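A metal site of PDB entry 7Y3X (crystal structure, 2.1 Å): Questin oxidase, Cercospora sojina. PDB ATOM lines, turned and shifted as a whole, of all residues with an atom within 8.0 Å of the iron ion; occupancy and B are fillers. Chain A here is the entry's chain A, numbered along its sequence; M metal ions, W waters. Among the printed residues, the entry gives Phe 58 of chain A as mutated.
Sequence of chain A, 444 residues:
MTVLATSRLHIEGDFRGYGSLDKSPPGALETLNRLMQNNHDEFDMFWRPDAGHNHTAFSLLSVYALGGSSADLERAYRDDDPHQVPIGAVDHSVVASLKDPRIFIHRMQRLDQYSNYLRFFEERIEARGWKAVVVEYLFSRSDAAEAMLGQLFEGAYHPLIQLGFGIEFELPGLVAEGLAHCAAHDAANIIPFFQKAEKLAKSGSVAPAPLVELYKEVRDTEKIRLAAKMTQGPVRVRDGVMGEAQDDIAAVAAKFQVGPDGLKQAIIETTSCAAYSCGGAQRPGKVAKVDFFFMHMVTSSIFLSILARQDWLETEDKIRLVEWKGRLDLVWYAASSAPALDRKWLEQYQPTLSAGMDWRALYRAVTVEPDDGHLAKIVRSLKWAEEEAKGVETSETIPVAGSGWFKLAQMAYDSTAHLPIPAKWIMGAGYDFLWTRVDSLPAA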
ATOM      1  N   ALA A  51     -36.322  20.511   5.547  1.00  0.00           N
ATOM      2  CA  ALA A  51     -35.112  20.242   6.345  1.00  0.00           C
ATOM      3  C   ALA A  51     -35.372  19.136   7.381  1.00  0.00           C
ATOM      4  O   ALA A  51     -34.755  19.171   8.473  1.00  0.00           O
ATOM      5  CB  ALA A  51     -34.628  21.512   6.987  1.00  0.00           C
ATOM      6  N   HIS A  53     -34.921  15.646   7.282  1.00  0.00           N
ATOM      7  CA  HIS A  53     -34.251  14.338   7.095  1.00  0.00           C
ATOM      8  C   HIS A  53     -33.828  13.775   8.461  1.00  0.00           C
ATOM      9  O   HIS A  53     -33.185  14.510   9.267  1.00  0.00           O
ATOM     10  CB  HIS A  53     -33.052  14.434   6.129  1.00  0.00           C
ATOM     11  CG  HIS A  53     -33.321  15.232   4.900  1.00  0.00           C
ATOM     12  ND1 HIS A  53     -33.108  16.594   4.842  1.00  0.00           N
ATOM     13  CD2 HIS A  53     -33.789  14.868   3.686  1.00  0.00           C
ATOM     14  CE1 HIS A  53     -33.424  17.031   3.647  1.00  0.00           C
ATOM     15  NE2 HIS A  53     -33.820  15.982   2.910  1.00  0.00           N
ATOM     16  N   ASN A  54     -34.189  12.516   8.715  1.00  0.00           N
ATOM     17  CA  ASN A  54     -33.749  11.745   9.914  1.00  0.00           C
ATOM     18  C   ASN A  54     -32.237  11.446   9.785  1.00  0.00           C
ATOM     19  O   ASN A  54     -31.841  10.662   8.900  1.00  0.00           O
ATOM     20  CB  ASN A  54     -34.557  10.468  10.076  1.00  0.00           C
ATOM     21  CG  ASN A  54     -34.118   9.635  11.256  1.00  0.00           C
ATOM     22  OD1 ASN A  54     -33.323  10.119  12.100  1.00  0.00           O
ATOM     23  ND2 ASN A  54     -34.591   8.389  11.288  1.00  0.00           N
ATOM     24  N   HIS A  55     -31.406  12.052  10.627  1.00  0.00           N
ATOM     25  CA  HIS A  55     -29.917  11.945  10.551  1.00  0.00           C
ATOM     26  C   HIS A  55     -29.359  10.803  11.421  1.00  0.00           C
ATOM     27  O   HIS A  55     -28.139  10.605  11.399  1.00  0.00           O
ATOM     28  CB  HIS A  55     -29.295  13.298  10.910  1.00  0.00           C
ATOM     29  CG  HIS A  55     -29.379  14.293   9.808  1.00  0.00           C
ATOM     30  ND1 HIS A  55     -30.597  14.820   9.375  1.00  0.00           N
ATOM     31  CD2 HIS A  55     -28.405  14.900   9.078  1.00  0.00           C
ATOM     32  CE1 HIS A  55     -30.351  15.698   8.411  1.00  0.00           C
ATOM     33  NE2 HIS A  55     -29.017  15.757   8.202  1.00  0.00           N
ATOM     34  N   PHE A  58     -26.847   8.479  10.006  1.00  0.00           N
ATOM     35  CA  PHE A  58     -25.641   9.214   9.594  1.00  0.00           C
ATOM     36  C   PHE A  58     -24.763   9.440  10.840  1.00  0.00           C
ATOM     37  O   PHE A  58     -23.515   9.292  10.790  1.00  0.00           O
ATOM     38  CB  PHE A  58     -26.002  10.534   8.896  1.00  0.00           C
ATOM     39  CG  PHE A  58     -27.119  10.466   7.865  1.00  0.00           C
ATOM     40  CD1 PHE A  58     -27.345   9.344   7.095  1.00  0.00           C
ATOM     41  CD2 PHE A  58     -27.931  11.566   7.652  1.00  0.00           C
ATOM     42  CE1 PHE A  58     -28.349   9.306   6.150  1.00  0.00           C
ATOM     43  CE2 PHE A  58     -28.942  11.538   6.699  1.00  0.00           C
ATOM     44  CZ  PHE A  58     -29.170  10.397   5.958  1.00  0.00           C
ATOM     45  N   HIS A  83     -35.278  13.996  15.570  1.00  0.00           N
ATOM     46  CA  HIS A  83     -35.319  13.475  14.177  1.00  0.00           C
ATOM     47  C   HIS A  83     -36.192  12.221  14.064  1.00  0.00           C
ATOM     48  O   HIS A  83     -36.353  11.726  12.930  1.00  0.00           O
ATOM     49  CB  HIS A  83     -33.908  13.193  13.685  1.00  0.00           C
ATOM     50  CG  HIS A  83     -33.068  14.398  13.435  1.00  0.00           C
ATOM     51  ND1 HIS A  83     -32.071  14.384  12.493  1.00  0.00           N
ATOM     52  CD2 HIS A  83     -33.065  15.627  13.977  1.00  0.00           C
ATOM     53  CE1 HIS A  83     -31.475  15.567  12.481  1.00  0.00           C
ATOM     54  NE2 HIS A  83     -32.086  16.361  13.377  1.00  0.00           N
ATOM     55  N   GLY A 155     -32.377  17.848  -1.475  1.00  0.00           N
ATOM     56  CA  GLY A 155     -32.345  18.210  -0.047  1.00  0.00           C
ATOM     57  C   GLY A 155     -30.936  18.547   0.420  1.00  0.00           C
ATOM     58  O   GLY A 155     -30.675  18.347   1.600  1.00  0.00           O
ATOM     59  N   ALA A 156     -30.049  19.011  -0.460  1.00  0.00           N
ATOM     60  CA  ALA A 156     -28.610  19.210  -0.191  1.00  0.00           C
ATOM     61  C   ALA A 156     -27.919  17.847   0.124  1.00  0.00           C
ATOM     62  O   ALA A 156     -27.130  17.784   1.077  1.00  0.00           O
ATOM     63  CB  ALA A 156     -28.406  20.218   0.938  1.00  0.00           C
ATOM     64  N   TYR A 157     -28.227  16.811  -0.664  1.00  0.00           N
ATOM     65  CA  TYR A 157     -27.445  15.549  -0.858  1.00  0.00           C
ATOM     66  C   TYR A 157     -27.826  14.466   0.161  1.00  0.00           C
ATOM     67  O   TYR A 157     -27.101  13.484   0.227  1.00  0.00           O
ATOM     68  CB  TYR A 157     -25.933  15.827  -0.870  1.00  0.00           C
ATOM     69  CG  TYR A 157     -25.519  16.894  -1.850  1.00  0.00           C
ATOM     70  CD1 TYR A 157     -25.731  16.726  -3.209  1.00  0.00           C
ATOM     71  CD2 TYR A 157     -24.957  18.077  -1.425  1.00  0.00           C
ATOM     72  CE1 TYR A 157     -25.396  17.712  -4.114  1.00  0.00           C
ATOM     73  CE2 TYR A 157     -24.566  19.056  -2.325  1.00  0.00           C
ATOM     74  CZ  TYR A 157     -24.799  18.877  -3.678  1.00  0.00           C
ATOM     75  OH  TYR A 157     -24.479  19.863  -4.584  1.00  0.00           O
ATOM     76  N   HIS A 158     -28.985  14.558   0.838  1.00  0.00           N
ATOM     77  CA  HIS A 158     -29.349  13.547   1.877  1.00  0.00           C
ATOM     78  C   HIS A 158     -29.558  12.144   1.276  1.00  0.00           C
ATOM     79  O   HIS A 158     -29.087  11.184   1.847  1.00  0.00           O
ATOM     80  CB  HIS A 158     -30.511  14.032   2.771  1.00  0.00           C
ATOM     81  CG  HIS A 158     -30.033  15.066   3.743  1.00  0.00           C
ATOM     82  ND1 HIS A 158     -30.117  16.433   3.476  1.00  0.00           N
ATOM     83  CD2 HIS A 158     -29.366  14.968   4.922  1.00  0.00           C
ATOM     84  CE1 HIS A 158     -29.548  17.111   4.443  1.00  0.00           C
ATOM     85  NE2 HIS A 158     -29.072  16.247   5.343  1.00  0.00           N
ATOM     86  N   ILE A 161     -26.149  10.738   0.461  1.00  0.00           N
ATOM     87  CA  ILE A 161     -25.437  10.466   1.737  1.00  0.00           C
ATOM     88  C   ILE A 161     -25.945   9.133   2.281  1.00  0.00           C
ATOM     89  O   ILE A 161     -25.095   8.302   2.635  1.00  0.00           O
ATOM     90  CB  ILE A 161     -25.593  11.629   2.724  1.00  0.00           C
ATOM     91  CG1 ILE A 161     -24.712  12.818   2.322  1.00  0.00           C
ATOM     92  CG2 ILE A 161     -25.274  11.121   4.107  1.00  0.00           C
ATOM     93  CD1 ILE A 161     -25.038  14.109   3.034  1.00  0.00           C
ATOM     94  N   PHE A 292     -24.025  26.141   6.520  1.00  0.00           N
ATOM     95  CA  PHE A 292     -24.745  24.861   6.739  1.00  0.00           C
ATOM     96  C   PHE A 292     -24.835  24.091   5.424  1.00  0.00           C
ATOM     97  O   PHE A 292     -24.659  22.856   5.415  1.00  0.00           O
ATOM     98  CB  PHE A 292     -26.140  25.157   7.296  1.00  0.00           C
ATOM     99  CG  PHE A 292     -27.039  23.979   7.554  1.00  0.00           C
ATOM    100  CD1 PHE A 292     -26.858  23.170   8.648  1.00  0.00           C
ATOM    101  CD2 PHE A 292     -28.110  23.712   6.714  1.00  0.00           C
ATOM    102  CE1 PHE A 292     -27.720  22.104   8.890  1.00  0.00           C
ATOM    103  CE2 PHE A 292     -28.957  22.637   6.957  1.00  0.00           C
ATOM    104  CZ  PHE A 292     -28.779  21.868   8.063  1.00  0.00           C
ATOM    105  N   MET A 295     -21.373  23.107   4.168  1.00  0.00           N
ATOM    106  CA  MET A 295     -21.039  21.923   5.022  1.00  0.00           C
ATOM    107  C   MET A 295     -21.572  20.621   4.398  1.00  0.00           C
ATOM    108  O   MET A 295     -20.843  19.579   4.453  1.00  0.00           O
ATOM    109  CB  MET A 295     -21.571  22.114   6.433  1.00  0.00           C
ATOM    110  CG  MET A 295     -21.368  20.896   7.349  1.00  0.00           C
ATOM    111  SD  MET A 295     -22.849  19.869   7.404  1.00  0.00           S
ATOM    112  CE  MET A 295     -23.947  21.072   8.150  1.00  0.00           C
ATOM    113  N   HIS A 296     -22.762  20.640   3.791  1.00  0.00           N
ATOM    114  CA  HIS A 296     -23.369  19.454   3.128  1.00  0.00           C
ATOM    115  C   HIS A 296     -22.626  19.158   1.823  1.00  0.00           C
ATOM    116  O   HIS A 296     -22.519  17.983   1.472  1.00  0.00           O
ATOM    117  CB  HIS A 296     -24.872  19.624   2.880  1.00  0.00           C
ATOM    118  CG  HIS A 296     -25.697  19.350   4.097  1.00  0.00           C
ATOM    119  ND1 HIS A 296     -25.896  20.289   5.076  1.00  0.00           N
ATOM    120  CD2 HIS A 296     -26.325  18.214   4.502  1.00  0.00           C
ATOM    121  CE1 HIS A 296     -26.629  19.747   6.043  1.00  0.00           C
ATOM    122  NE2 HIS A 296     -26.866  18.445   5.720  1.00  0.00           N
ATOM    123  N   THR A 299     -19.779  17.325   3.346  1.00  0.00           N
ATOM    124  CA  THR A 299     -20.091  16.027   3.997  1.00  0.00           C
ATOM    125  C   THR A 299     -20.463  14.984   2.948  1.00  0.00           C
ATOM    126  O   THR A 299     -20.129  13.799   3.155  1.00  0.00           O
ATOM    127  CB  THR A 299     -21.180  16.123   5.063  1.00  0.00           C
ATOM    128  OG1 THR A 299     -22.407  16.478   4.416  1.00  0.00           O
ATOM    129  CG2 THR A 299     -20.801  17.069   6.180  1.00  0.00           C
ATOM    130  N   ASP A 372     -26.076  16.631  16.010  1.00  0.00           N
ATOM    131  CA  ASP A 372     -27.064  15.830  15.228  1.00  0.00           C
ATOM    132  C   ASP A 372     -26.368  14.906  14.246  1.00  0.00           C
ATOM    133  O   ASP A 372     -27.063  14.136  13.593  1.00  0.00           O
ATOM    134  CB  ASP A 372     -28.033  16.747  14.507  1.00  0.00           C
ATOM    135  CG  ASP A 372     -27.456  17.879  13.672  1.00  0.00           C
ATOM    136  OD1 ASP A 372     -26.229  17.943  13.461  1.00  0.00           O
ATOM    137  OD2 ASP A 372     -28.266  18.690  13.273  1.00  0.00           O
ATOM    138  N   GLY A 373     -25.035  15.009  14.099  1.00  0.00           N
ATOM    139  CA  GLY A 373     -24.203  14.138  13.246  1.00  0.00           C
ATOM    140  C   GLY A 373     -23.382  14.944  12.246  1.00  0.00           C
ATOM    141  O   GLY A 373     -22.418  14.375  11.674  1.00  0.00           O
ATOM    142  N   HIS A 374     -23.711  16.218  12.000  1.00  0.00           N
ATOM    143  CA  HIS A 374     -22.996  16.976  10.937  1.00  0.00           C
ATOM    144  C   HIS A 374     -21.516  17.181  11.301  1.00  0.00           C
ATOM    145  O   HIS A 374     -20.693  17.248  10.356  1.00  0.00           O
ATOM    146  CB  HIS A 374     -23.671  18.318  10.610  1.00  0.00           C
ATOM    147  CG  HIS A 374     -25.006  18.158   9.985  1.00  0.00           C
ATOM    148  ND1 HIS A 374     -26.168  18.413  10.690  1.00  0.00           N
ATOM    149  CD2 HIS A 374     -25.364  17.739   8.761  1.00  0.00           C
ATOM    150  CE1 HIS A 374     -27.210  18.180   9.900  1.00  0.00           C
ATOM    151  NE2 HIS A 374     -26.737  17.745   8.694  1.00  0.00           N
ATOM    152  N   KCX A 377     -19.716  14.018  10.521  1.00  0.00           N
ATOM    153  CA  KCX A 377     -19.756  13.864   9.040  1.00  0.00           C
ATOM    154  CB  KCX A 377     -21.133  14.226   8.481  1.00  0.00           C
ATOM    155  CG  KCX A 377     -22.251  13.230   8.777  1.00  0.00           C
ATOM    156  CD  KCX A 377     -23.135  13.075   7.556  1.00  0.00           C
ATOM    157  CE  KCX A 377     -24.521  13.477   7.832  1.00  0.00           C
ATOM    158  NZ  KCX A 377     -25.172  13.956   6.630  1.00  0.00           N
ATOM    159  C   KCX A 377     -18.713  14.779   8.394  1.00  0.00           C
ATOM    160  O   KCX A 377     -17.985  14.302   7.501  1.00  0.00           O
ATOM    161  CX  KCX A 377     -25.311  15.270   6.376  1.00  0.00           C
ATOM    162  OQ1 KCX A 377     -24.402  16.045   6.094  1.00  0.00           O
ATOM    163  OQ2 KCX A 377     -26.571  15.603   6.537  1.00  0.00           O
HETATM  164 FE    FE M   1     -27.816  17.102   6.946  1.00  0.00          FE
HETATM  165  O   HOH W   1     -29.473  18.575   7.473  1.00  0.00           O
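ND1 of His 158 sits at hydrogen-bond distance from O of Gly 155 (2.7 Å).
The backbone NH of His 55 lies within hydrogen-bond range of a ring nitrogen (ND1) of His 83.
OQ1 of KCX 377 sits at hydrogen-bond distance from OG1 of Thr 299 (2.6 Å).
The backbone carbonyl oxygen (O) of His 53 is in hydrogen-bond range of a ring nitrogen (ND1) of His 55, 2.6 Å away.
A ring nitrogen (ND1) of His 374 is in hydrogen-bond range of the side-chain carboxylate of Asp 372 (2.8 Å).
The backbone carbonyl oxygen (O) of Phe 292 is in hydrogen-bond range of a ring nitrogen (ND1) of His 296, at 2.9 Å.
A ring nitrogen (ND1) of His 53 lies within hydrogen-bond range of a ring nitrogen (ND1) of His 158.
The backbone carbonyl oxygen of His 296 sits at hydrogen-bond distance from the side-chain hydroxyl of Thr 299, 3.3 Å away.
Five residues have an atom within 4 Å of the iron ion: His 55, His 158, His 296, His 374 and KCX 377.
The nearest printed residue that does not touch the iron ion is Phe 292 (5.0 Å).
The iron ion is bound by OQ2 of KCX 377 (2.0 Å), a ring nitrogen (NE2) of His 296 (2.1 Å), a ring nitrogen (NE2) of His 374 (2.2 Å), a ring nitrogen (NE2) of His 55 (2.2 Å), a ring nitrogen (NE2) of His 158 (2.2 Å) and water W1 (2.3 Å).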
